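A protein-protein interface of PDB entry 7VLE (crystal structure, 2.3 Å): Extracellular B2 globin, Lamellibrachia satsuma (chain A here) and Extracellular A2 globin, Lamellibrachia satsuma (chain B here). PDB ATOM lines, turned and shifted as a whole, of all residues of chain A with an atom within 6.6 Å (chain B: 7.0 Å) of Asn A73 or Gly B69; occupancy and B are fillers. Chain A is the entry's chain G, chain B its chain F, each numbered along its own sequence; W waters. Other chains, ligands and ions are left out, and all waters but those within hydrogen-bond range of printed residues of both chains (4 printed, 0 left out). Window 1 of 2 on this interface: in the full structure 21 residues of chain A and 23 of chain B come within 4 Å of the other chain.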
ATOM      1  N   TRP A  17      33.734 -26.297   9.189  1.00  0.00           N
ATOM      2  CA  TRP A  17      33.794 -25.156  10.092  1.00  0.00           C
ATOM      3  C   TRP A  17      33.869 -25.603  11.545  1.00  0.00           C
ATOM      4  O   TRP A  17      34.593 -25.000  12.347  1.00  0.00           O
ATOM      5  CB  TRP A  17      32.571 -24.269   9.864  1.00  0.00           C
ATOM      6  CG  TRP A  17      32.657 -22.939  10.513  1.00  0.00           C
ATOM      7  CD1 TRP A  17      31.833 -22.444  11.478  1.00  0.00           C
ATOM      8  CD2 TRP A  17      33.624 -21.921  10.247  1.00  0.00           C
ATOM      9  NE1 TRP A  17      32.225 -21.177  11.830  1.00  0.00           N
ATOM     10  CE2 TRP A  17      33.324 -20.832  11.088  1.00  0.00           C
ATOM     11  CE3 TRP A  17      34.715 -21.822   9.378  1.00  0.00           C
ATOM     12  CZ2 TRP A  17      34.075 -19.659  11.086  1.00  0.00           C
ATOM     13  CZ3 TRP A  17      35.460 -20.660   9.377  1.00  0.00           C
ATOM     14  CH2 TRP A  17      35.137 -19.594  10.225  1.00  0.00           C
ATOM     15  N   TRP A  21      36.647 -24.461  14.484  1.00  0.00           N
ATOM     16  CA  TRP A  21      36.200 -23.387  15.367  1.00  0.00           C
ATOM     17  C   TRP A  21      36.434 -23.727  16.837  1.00  0.00           C
ATOM     18  O   TRP A  21      36.051 -24.802  17.309  1.00  0.00           O
ATOM     19  CB  TRP A  21      34.718 -23.126  15.095  1.00  0.00           C
ATOM     20  CG  TRP A  21      33.945 -22.431  16.175  1.00  0.00           C
ATOM     21  CD1 TRP A  21      33.445 -22.989  17.319  1.00  0.00           C
ATOM     22  CD2 TRP A  21      33.530 -21.062  16.183  1.00  0.00           C
ATOM     23  NE1 TRP A  21      32.771 -22.043  18.051  1.00  0.00           N
ATOM     24  CE2 TRP A  21      32.806 -20.852  17.375  1.00  0.00           C
ATOM     25  CE3 TRP A  21      33.711 -19.987  15.307  1.00  0.00           C
ATOM     26  CZ2 TRP A  21      32.264 -19.614  17.710  1.00  0.00           C
ATOM     27  CZ3 TRP A  21      33.173 -18.760  15.643  1.00  0.00           C
ATOM     28  CH2 TRP A  21      32.458 -18.583  16.833  1.00  0.00           C
ATOM     29  N   ARG A  29      40.371 -18.887  16.518  1.00  0.00           N
ATOM     30  CA  ARG A  29      39.580 -17.980  15.692  1.00  0.00           C
ATOM     31  C   ARG A  29      40.439 -16.862  15.120  1.00  0.00           C
ATOM     32  O   ARG A  29      40.317 -16.511  13.940  1.00  0.00           O
ATOM     33  CB  ARG A  29      38.442 -17.374  16.511  1.00  0.00           C
ATOM     34  CG  ARG A  29      37.566 -18.357  17.256  1.00  0.00           C
ATOM     35  CD  ARG A  29      36.438 -17.606  17.944  1.00  0.00           C
ATOM     36  NE  ARG A  29      35.652 -18.455  18.830  1.00  0.00           N
ATOM     37  CZ  ARG A  29      34.599 -18.034  19.522  1.00  0.00           C
ATOM     38  NH1 ARG A  29      34.201 -16.773  19.426  1.00  0.00           N
ATOM     39  NH2 ARG A  29      33.940 -18.875  20.308  1.00  0.00           N
ATOM     40  N   CYS A  68      38.583  -8.872  13.308  1.00  0.00           N
ATOM     41  CA  CYS A  68      38.743 -10.270  12.923  1.00  0.00           C
ATOM     42  C   CYS A  68      37.781 -11.178  13.683  1.00  0.00           C
ATOM     43  O   CYS A  68      37.134 -12.053  13.095  1.00  0.00           O
ATOM     44  CB  CYS A  68      40.187 -10.710  13.174  1.00  0.00           C
ATOM     45  SG  CYS A  68      41.358 -10.180  11.913  1.00  0.00           S
ATOM     46  N   ILE A  69      37.693 -10.995  15.001  1.00  0.00           N
ATOM     47  CA  ILE A  69      36.790 -11.807  15.811  1.00  0.00           C
ATOM     48  C   ILE A  69      35.340 -11.509  15.453  1.00  0.00           C
ATOM     49  O   ILE A  69      34.488 -12.406  15.447  1.00  0.00           O
ATOM     50  CB  ILE A  69      37.081 -11.574  17.306  1.00  0.00           C
ATOM     51  CG1 ILE A  69      38.399 -12.250  17.693  1.00  0.00           C
ATOM     52  CG2 ILE A  69      35.934 -12.069  18.177  1.00  0.00           C
ATOM     53  CD1 ILE A  69      38.892 -11.881  19.064  1.00  0.00           C
ATOM     54  N   ARG A  70      35.038 -10.248  15.131  1.00  0.00           N
ATOM     55  CA  ARG A  70      33.697  -9.905  14.671  1.00  0.00           C
ATOM     56  C   ARG A  70      33.394 -10.535  13.316  1.00  0.00           C
ATOM     57  O   ARG A  70      32.258 -10.948  13.060  1.00  0.00           O
ATOM     58  CB  ARG A  70      33.537  -8.384  14.600  1.00  0.00           C
ATOM     59  CG  ARG A  70      33.344  -7.706  15.946  1.00  0.00           C
ATOM     60  CD  ARG A  70      32.856  -6.274  15.776  1.00  0.00           C
ATOM     61  NE  ARG A  70      33.839  -5.423  15.109  1.00  0.00           N
ATOM     62  CZ  ARG A  70      34.792  -4.747  15.741  1.00  0.00           C
ATOM     63  NH1 ARG A  70      34.899  -4.825  17.062  1.00  0.00           N
ATOM     64  NH2 ARG A  70      35.643  -3.995  15.056  1.00  0.00           N
ATOM     65  N   VAL A  71      34.399 -10.623  12.441  1.00  0.00           N
ATOM     66  CA  VAL A  71      34.184 -11.163  11.099  1.00  0.00           C
ATOM     67  C   VAL A  71      33.848 -12.646  11.164  1.00  0.00           C
ATOM     68  O   VAL A  71      32.843 -13.096  10.600  1.00  0.00           O
ATOM     69  CB  VAL A  71      35.416 -10.921  10.210  1.00  0.00           C
ATOM     70  CG1 VAL A  71      35.266 -11.673   8.895  1.00  0.00           C
ATOM     71  CG2 VAL A  71      35.604  -9.449   9.949  1.00  0.00           C
ATOM     72  N   VAL A  72      34.702 -13.434  11.824  1.00  0.00           N
ATOM     73  CA  VAL A  72      34.481 -14.876  11.887  1.00  0.00           C
ATOM     74  C   VAL A  72      33.199 -15.186  12.640  1.00  0.00           C
ATOM     75  O   VAL A  72      32.534 -16.191  12.359  1.00  0.00           O
ATOM     76  CB  VAL A  72      35.692 -15.588  12.522  1.00  0.00           C
ATOM     77  CG1 VAL A  72      36.890 -15.537  11.589  1.00  0.00           C
ATOM     78  CG2 VAL A  72      36.029 -14.974  13.870  1.00  0.00           C
ATOM     79  N   ASN A  73      32.832 -14.341  13.606  1.00  0.00           N
ATOM     80  CA  ASN A  73      31.546 -14.501  14.272  1.00  0.00           C
ATOM     81  C   ASN A  73      30.399 -14.295  13.293  1.00  0.00           C
ATOM     82  O   ASN A  73      29.374 -14.983  13.371  1.00  0.00           O
ATOM     83  CB  ASN A  73      31.434 -13.526  15.442  1.00  0.00           C
ATOM     84  CG  ASN A  73      30.062 -13.544  16.084  1.00  0.00           C
ATOM     85  OD1 ASN A  73      29.710 -14.487  16.792  1.00  0.00           O
ATOM     86  ND2 ASN A  73      29.280 -12.498  15.842  1.00  0.00           N
ATOM     87  N   GLY A  74      30.556 -13.352  12.362  1.00  0.00           N
ATOM     88  CA  GLY A  74      29.533 -13.139  11.355  1.00  0.00           C
ATOM     89  C   GLY A  74      29.457 -14.262  10.342  1.00  0.00           C
ATOM     90  O   GLY A  74      28.372 -14.588   9.854  1.00  0.00           O
ATOM     91  N   LEU A  75      30.600 -14.864  10.008  1.00  0.00           N
ATOM     92  CA  LEU A  75      30.594 -16.021   9.120  1.00  0.00           C
ATOM     93  C   LEU A  75      30.038 -17.249   9.829  1.00  0.00           C
ATOM     94  O   LEU A  75      29.276 -18.024   9.239  1.00  0.00           O
ATOM     95  CB  LEU A  75      32.007 -16.290   8.603  1.00  0.00           C
ATOM     96  CG  LEU A  75      32.190 -17.506   7.694  1.00  0.00           C
ATOM     97  CD1 LEU A  75      31.342 -17.365   6.440  1.00  0.00           C
ATOM     98  CD2 LEU A  75      33.658 -17.699   7.338  1.00  0.00           C
ATOM     99  N   ASP A  76      30.407 -17.434  11.099  1.00  0.00           N
ATOM    100  CA  ASP A  76      29.894 -18.559  11.876  1.00  0.00           C
ATOM    101  C   ASP A  76      28.386 -18.462  12.058  1.00  0.00           C
ATOM    102  O   ASP A  76      27.679 -19.476  11.991  1.00  0.00           O
ATOM    103  CB  ASP A  76      30.598 -18.613  13.231  1.00  0.00           C
ATOM    104  CG  ASP A  76      30.084 -19.732  14.108  1.00  0.00           C
ATOM    105  OD1 ASP A  76      29.271 -19.459  15.016  1.00  0.00           O
ATOM    106  OD2 ASP A  76      30.484 -20.890  13.876  1.00  0.00           O
ATOM    107  N   SER A  77      27.875 -17.254  12.300  1.00  0.00           N
ATOM    108  CA  SER A  77      26.430 -17.069  12.383  1.00  0.00           C
ATOM    109  C   SER A  77      25.767 -17.410  11.057  1.00  0.00           C
ATOM    110  O   SER A  77      24.659 -17.957  11.027  1.00  0.00           O
ATOM    111  CB  SER A  77      26.104 -15.630  12.784  1.00  0.00           C
ATOM    112  OG  SER A  77      26.080 -14.783  11.648  1.00  0.00           O
ATOM    113  N   ALA A  78      26.440 -17.098   9.949  1.00  0.00           N
ATOM    114  CA  ALA A  78      25.903 -17.401   8.628  1.00  0.00           C
ATOM    115  C   ALA A  78      25.977 -18.894   8.334  1.00  0.00           C
ATOM    116  O   ALA A  78      25.006 -19.491   7.855  1.00  0.00           O
ATOM    117  CB  ALA A  78      26.658 -16.602   7.566  1.00  0.00           C
ATOM    118  N   GLN A  91      19.627 -12.457   8.501  1.00  0.00           N
ATOM    119  CA  GLN A  91      20.953 -12.132   9.018  1.00  0.00           C
ATOM    120  C   GLN A  91      21.852 -11.583   7.919  1.00  0.00           C
ATOM    121  O   GLN A  91      22.628 -10.648   8.152  1.00  0.00           O
ATOM    122  CB  GLN A  91      21.581 -13.371   9.657  1.00  0.00           C
ATOM    123  CG  GLN A  91      23.039 -13.205  10.066  1.00  0.00           C
ATOM    124  CD  GLN A  91      23.213 -12.339  11.299  1.00  0.00           C
ATOM    125  OE1 GLN A  91      22.239 -11.880  11.894  1.00  0.00           O
ATOM    126  NE2 GLN A  91      24.462 -12.117  11.691  1.00  0.00           N
ATOM    127  N   TRP B  15      29.526 -21.941  28.993  1.00  0.00           N
ATOM    128  CA  TRP B  15      28.952 -21.279  27.826  1.00  0.00           C
ATOM    129  C   TRP B  15      29.046 -22.172  26.597  1.00  0.00           C
ATOM    130  O   TRP B  15      28.063 -22.356  25.871  1.00  0.00           O
ATOM    131  CB  TRP B  15      29.653 -19.946  27.569  1.00  0.00           C
ATOM    132  CG  TRP B  15      29.313 -19.348  26.237  1.00  0.00           C
ATOM    133  CD1 TRP B  15      30.084 -19.357  25.110  1.00  0.00           C
ATOM    134  CD2 TRP B  15      28.104 -18.665  25.892  1.00  0.00           C
ATOM    135  NE1 TRP B  15      29.430 -18.715  24.085  1.00  0.00           N
ATOM    136  CE2 TRP B  15      28.212 -18.281  24.540  1.00  0.00           C
ATOM    137  CE3 TRP B  15      26.941 -18.338  26.595  1.00  0.00           C
ATOM    138  CZ2 TRP B  15      27.202 -17.586  23.879  1.00  0.00           C
ATOM    139  CZ3 TRP B  15      25.941 -17.649  25.938  1.00  0.00           C
ATOM    140  CH2 TRP B  15      26.077 -17.281  24.595  1.00  0.00           C
ATOM    141  N   TYR B  19      25.843 -22.940  24.557  1.00  0.00           N
ATOM    142  CA  TYR B  19      25.835 -22.380  23.209  1.00  0.00           C
ATOM    143  C   TYR B  19      25.992 -23.473  22.162  1.00  0.00           C
ATOM    144  O   TYR B  19      25.383 -23.410  21.088  1.00  0.00           O
ATOM    145  CB  TYR B  19      26.948 -21.341  23.084  1.00  0.00           C
ATOM    146  CG  TYR B  19      26.828 -20.409  21.904  1.00  0.00           C
ATOM    147  CD1 TYR B  19      25.594 -19.908  21.510  1.00  0.00           C
ATOM    148  CD2 TYR B  19      27.954 -20.004  21.202  1.00  0.00           C
ATOM    149  CE1 TYR B  19      25.486 -19.044  20.434  1.00  0.00           C
ATOM    150  CE2 TYR B  19      27.856 -19.142  20.129  1.00  0.00           C
ATOM    151  CZ  TYR B  19      26.621 -18.664  19.748  1.00  0.00           C
ATOM    152  OH  TYR B  19      26.525 -17.804  18.678  1.00  0.00           O
ATOM    153  N   ARG B  25      21.038 -23.711  18.931  1.00  0.00           N
ATOM    154  CA  ARG B  25      21.153 -22.284  19.210  1.00  0.00           C
ATOM    155  C   ARG B  25      19.817 -21.567  19.063  1.00  0.00           C
ATOM    156  O   ARG B  25      19.566 -20.580  19.765  1.00  0.00           O
ATOM    157  CB  ARG B  25      22.199 -21.649  18.291  1.00  0.00           C
ATOM    158  CG  ARG B  25      23.636 -22.003  18.648  1.00  0.00           C
ATOM    159  CD  ARG B  25      24.635 -21.324  17.718  1.00  0.00           C
ATOM    160  NE  ARG B  25      26.014 -21.655  18.071  1.00  0.00           N
ATOM    161  CZ  ARG B  25      27.076 -21.323  17.343  1.00  0.00           C
ATOM    162  NH1 ARG B  25      26.926 -20.650  16.211  1.00  0.00           N
ATOM    163  NH2 ARG B  25      28.292 -21.669  17.747  1.00  0.00           N
ATOM    164  N   HIS B  63      18.003 -11.503  14.995  1.00  0.00           N
ATOM    165  CA  HIS B  63      18.511 -10.597  16.021  1.00  0.00           C
ATOM    166  C   HIS B  63      19.056 -11.369  17.214  1.00  0.00           C
ATOM    167  O   HIS B  63      20.145 -11.069  17.717  1.00  0.00           O
ATOM    168  CB  HIS B  63      17.416  -9.637  16.481  1.00  0.00           C
ATOM    169  CG  HIS B  63      17.763  -8.904  17.739  1.00  0.00           C
ATOM    170  ND1 HIS B  63      18.705  -7.899  17.774  1.00  0.00           N
ATOM    171  CD2 HIS B  63      17.321  -9.050  19.009  1.00  0.00           C
ATOM    172  CE1 HIS B  63      18.817  -7.445  19.010  1.00  0.00           C
ATOM    173  NE2 HIS B  63      17.987  -8.127  19.779  1.00  0.00           N
ATOM    174  N   ALA B  64      18.292 -12.352  17.697  1.00  0.00           N
ATOM    175  CA  ALA B  64      18.764 -13.190  18.793  1.00  0.00           C
ATOM    176  C   ALA B  64      20.078 -13.868  18.433  1.00  0.00           C
ATOM    177  O   ALA B  64      20.959 -14.029  19.288  1.00  0.00           O
ATOM    178  CB  ALA B  64      17.701 -14.227  19.152  1.00  0.00           C
ATOM    179  N   THR B  65      20.226 -14.270  17.167  1.00  0.00           N
ATOM    180  CA  THR B  65      21.497 -14.807  16.691  1.00  0.00           C
ATOM    181  C   THR B  65      22.629 -13.811  16.908  1.00  0.00           C
ATOM    182  O   THR B  65      23.718 -14.185  17.361  1.00  0.00           O
ATOM    183  CB  THR B  65      21.384 -15.170  15.210  1.00  0.00           C
ATOM    184  OG1 THR B  65      20.494 -16.282  15.050  1.00  0.00           O
ATOM    185  CG2 THR B  65      22.748 -15.520  14.630  1.00  0.00           C
ATOM    186  N   ARG B  66      22.387 -12.537  16.595  1.00  0.00           N
ATOM    187  CA  ARG B  66      23.417 -11.518  16.762  1.00  0.00           C
ATOM    188  C   ARG B  66      23.748 -11.295  18.233  1.00  0.00           C
ATOM    189  O   ARG B  66      24.920 -11.131  18.592  1.00  0.00           O
ATOM    190  CB  ARG B  66      22.970 -10.207  16.114  1.00  0.00           C
ATOM    191  CG  ARG B  66      22.803 -10.283  14.607  1.00  0.00           C
ATOM    192  CD  ARG B  66      22.579  -8.906  14.001  1.00  0.00           C
ATOM    193  NE  ARG B  66      21.219  -8.417  14.203  1.00  0.00           N
ATOM    194  CZ  ARG B  66      20.209  -8.662  13.374  1.00  0.00           C
ATOM    195  NH1 ARG B  66      19.001  -8.176  13.629  1.00  0.00           N
ATOM    196  NH2 ARG B  66      20.405  -9.401  12.291  1.00  0.00           N
ATOM    197  N   VAL B  67      22.726 -11.283  19.093  1.00  0.00           N
ATOM    198  CA  VAL B  67      22.940 -11.057  20.523  1.00  0.00           C
ATOM    199  C   VAL B  67      23.830 -12.145  21.104  1.00  0.00           C
ATOM    200  O   VAL B  67      24.862 -11.866  21.729  1.00  0.00           O
ATOM    201  CB  VAL B  67      21.597 -10.998  21.268  1.00  0.00           C
ATOM    202  CG1 VAL B  67      21.836 -10.829  22.759  1.00  0.00           C
ATOM    203  CG2 VAL B  67      20.731  -9.879  20.725  1.00  0.00           C
ATOM    204  N   LEU B  68      23.423 -13.406  20.930  1.00  0.00           N
ATOM    205  CA  LEU B  68      24.207 -14.519  21.456  1.00  0.00           C
ATOM    206  C   LEU B  68      25.599 -14.543  20.843  1.00  0.00           C
ATOM    207  O   LEU B  68      26.574 -14.908  21.512  1.00  0.00           O
ATOM    208  CB  LEU B  68      23.491 -15.844  21.195  1.00  0.00           C
ATOM    209  CG  LEU B  68      22.030 -16.003  21.622  1.00  0.00           C
ATOM    210  CD1 LEU B  68      21.658 -17.478  21.650  1.00  0.00           C
ATOM    211  CD2 LEU B  68      21.759 -15.347  22.968  1.00  0.00           C
ATOM    212  N   GLY B  69      25.709 -14.166  19.569  1.00  0.00           N
ATOM    213  CA  GLY B  69      27.020 -14.019  18.965  1.00  0.00           C
ATOM    214  C   GLY B  69      27.852 -12.955  19.656  1.00  0.00           C
ATOM    215  O   GLY B  69      29.064 -13.112  19.824  1.00  0.00           O
ATOM    216  N   GLY B  70      27.209 -11.862  20.072  1.00  0.00           N
ATOM    217  CA  GLY B  70      27.916 -10.857  20.848  1.00  0.00           C
ATOM    218  C   GLY B  70      28.381 -11.388  22.190  1.00  0.00           C
ATOM    219  O   GLY B  70      29.516 -11.141  22.606  1.00  0.00           O
ATOM    220  N   LEU B  71      27.513 -12.133  22.880  1.00  0.00           N
ATOM    221  CA  LEU B  71      27.894 -12.748  24.149  1.00  0.00           C
ATOM    222  C   LEU B  71      29.027 -13.746  23.964  1.00  0.00           C
ATOM    223  O   LEU B  71      29.950 -13.809  24.784  1.00  0.00           O
ATOM    224  CB  LEU B  71      26.686 -13.439  24.778  1.00  0.00           C
ATOM    225  CG  LEU B  71      25.735 -12.554  25.575  1.00  0.00           C
ATOM    226  CD1 LEU B  71      24.489 -13.334  25.954  1.00  0.00           C
ATOM    227  CD2 LEU B  71      26.446 -12.037  26.810  1.00  0.00           C
ATOM    228  N   ASP B  72      28.963 -14.546  22.897  1.00  0.00           N
ATOM    229  CA  ASP B  72      30.002 -15.536  22.638  1.00  0.00           C
ATOM    230  C   ASP B  72      31.364 -14.876  22.474  1.00  0.00           C
ATOM    231  O   ASP B  72      32.366 -15.357  23.021  1.00  0.00           O
ATOM    232  CB  ASP B  72      29.638 -16.349  21.395  1.00  0.00           C
ATOM    233  CG  ASP B  72      30.663 -17.416  21.074  1.00  0.00           C
ATOM    234  OD1 ASP B  72      31.527 -17.179  20.205  1.00  0.00           O
ATOM    235  OD2 ASP B  72      30.611 -18.491  21.707  1.00  0.00           O
ATOM    236  N   MET B  73      31.417 -13.767  21.732  1.00  0.00           N
ATOM    237  CA  MET B  73      32.677 -13.060  21.529  1.00  0.00           C
ATOM    238  C   MET B  73      33.262 -12.571  22.849  1.00  0.00           C
ATOM    239  O   MET B  73      34.468 -12.703  23.087  1.00  0.00           O
ATOM    240  CB  MET B  73      32.470 -11.890  20.563  1.00  0.00           C
ATOM    241  CG  MET B  73      32.216 -12.307  19.117  1.00  0.00           C
ATOM    242  SD  MET B  73      32.195 -10.926  17.951  1.00  0.00           S
ATOM    243  CE  MET B  73      30.685 -10.092  18.434  1.00  0.00           C
ATOM    244  N   CYS B  74      32.421 -12.007  23.720  1.00  0.00           N
ATOM    245  CA  CYS B  74      32.893 -11.547  25.024  1.00  0.00           C
ATOM    246  C   CYS B  74      33.394 -12.710  25.868  1.00  0.00           C
ATOM    247  O   CYS B  74      34.449 -12.623  26.509  1.00  0.00           O
ATOM    248  CB  CYS B  74      31.776 -10.807  25.760  1.00  0.00           C
ATOM    249  SG  CYS B  74      31.185  -9.310  24.959  1.00  0.00           S
ATOM    250  N   GLN B  87      36.175  -5.022  22.336  1.00  0.00           N
ATOM    251  CA  GLN B  87      34.880  -5.520  21.888  1.00  0.00           C
ATOM    252  C   GLN B  87      33.754  -5.005  22.775  1.00  0.00           C
ATOM    253  O   GLN B  87      32.655  -4.718  22.287  1.00  0.00           O
ATOM    254  CB  GLN B  87      34.895  -7.048  21.864  1.00  0.00           C
ATOM    255  CG  GLN B  87      33.586  -7.674  21.431  1.00  0.00           C
ATOM    256  CD  GLN B  87      33.187  -7.267  20.029  1.00  0.00           C
ATOM    257  OE1 GLN B  87      34.036  -7.090  19.155  1.00  0.00           O
ATOM    258  NE2 GLN B  87      31.887  -7.109  19.807  1.00  0.00           N
HETATM  259  O   HOH W   1      30.142 -23.261  15.490  1.00  0.00           O
HETATM  260  O   HOH W   2      26.828 -10.629  16.945  1.00  0.00           O
HETATM  261  O   HOH W   3      33.032 -18.570  23.328  1.00  0.00           O
HETATM  262  O   HOH W   4      29.044 -17.508  17.216  1.00  0.00           O
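NH1 of Arg B25 is in salt-bridge range of OD1 of Asp A76, 2.9 Å away. The guanidinium group of Arg B66 sits at hydrogen-bond distance from the side-chain amide oxygen of Gln A91, at 3.1 Å. The backbone carbonyl oxygen (O) of Gly B69 sits close to the side-chain amide oxygen (OD1) of Asn A73 (3.4 Å). NH1 of Arg A29 lies within salt-bridge range of OD1 of Asp B72, 2.8 Å away. The side-chain amide oxygen (OE1) of Gln B87 is in hydrogen-bond range of the guanidinium group (NH1) of Arg A70 (3.2 Å). The backbone carbonyl oxygen of Ile A69 sits close to the side-chain sulfur of Met B73.
Of the 16 printed residues of chain B, 7 touch a printed residue of chain A. Printed residues of chain B that touch a printed residue of chain A: Arg B25, Thr B65, Arg B66, Gly B69, Asp B72, Met B73 and Gln B87. Of the 15 printed residues of chain A, 8 touch a printed residue of chain B. Among the printed residues, Asp or Glu carboxylates within 4 Å of a Lys or Arg side-chain nitrogen of the other chain: Arg A29 with Asp B72 and Asp A76 with Arg B25.
The indole nitrogen (NE1) of Trp B15 is in hydrogen-bond range of the side-chain carboxylate (OD2) of Asp B72. The indole nitrogen of Trp A17 sits at hydrogen-bond distance from the side-chain carboxylate of Asp A76, at 2.7 Å. The backbone carbonyl oxygen (O) of Gly A74 sits at hydrogen-bond distance from the side-chain hydroxyl (OG) of Ser A77, 2.9 Å away. NE2 of Gln A91 sits at hydrogen-bond distance from OG of Ser A77 (3.1 Å).
Water W2 lies within hydrogen-bond range of O of Arg B66 (2.6 Å), ND2 of Asn A73 (3.3 Å) and N of Gly B70 (3.4 Å). Water W1 bridges the side-chain carboxylate of Asp A76 (2.9 Å) and the guanidinium group of Arg B25 (3.3 Å). Water W3 bridges the side-chain carboxylate (OD2) of Asp B72 (2.9 Å) and the guanidinium group (NH2) of Arg A29 (3.2 Å). Water W4 lies within hydrogen-bond range of OH of Tyr B19 (2.9 Å), OD1 of Asp A76 (2.9 Å) and OD1 of Asn A73 (3.1 Å).
Asn A73 touches just these residues of chain B: Gly B69 (3.4 Å) and Met B73 (3.7 Å). Ala A78 touches none of the printed residues of chain B. His B63 touches none of the printed residues of chain A. Printed residues of chain A within 4 Å of Arg B66: Gln A91 (3.1 Å). Printed residues of chain A within 4 Å of Gly B69: Asn A73 (3.4 Å). Of the printed residues of chain A, Met B73 touches Ile A69, Arg A70 and Asn A73. The nearest printed residue of chain A that does not touch Arg B25 is Trp A21 (4.5 Å).
Among the printed residues, pairs that only touch across the chains: Trp A21 with Asp B72 (3.6 Å), Asn A73 with Met B73 (3.7 Å), Arg A70 with Met B73 (3.7 Å) and Ser A77 with Thr B65 (3.8 Å).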
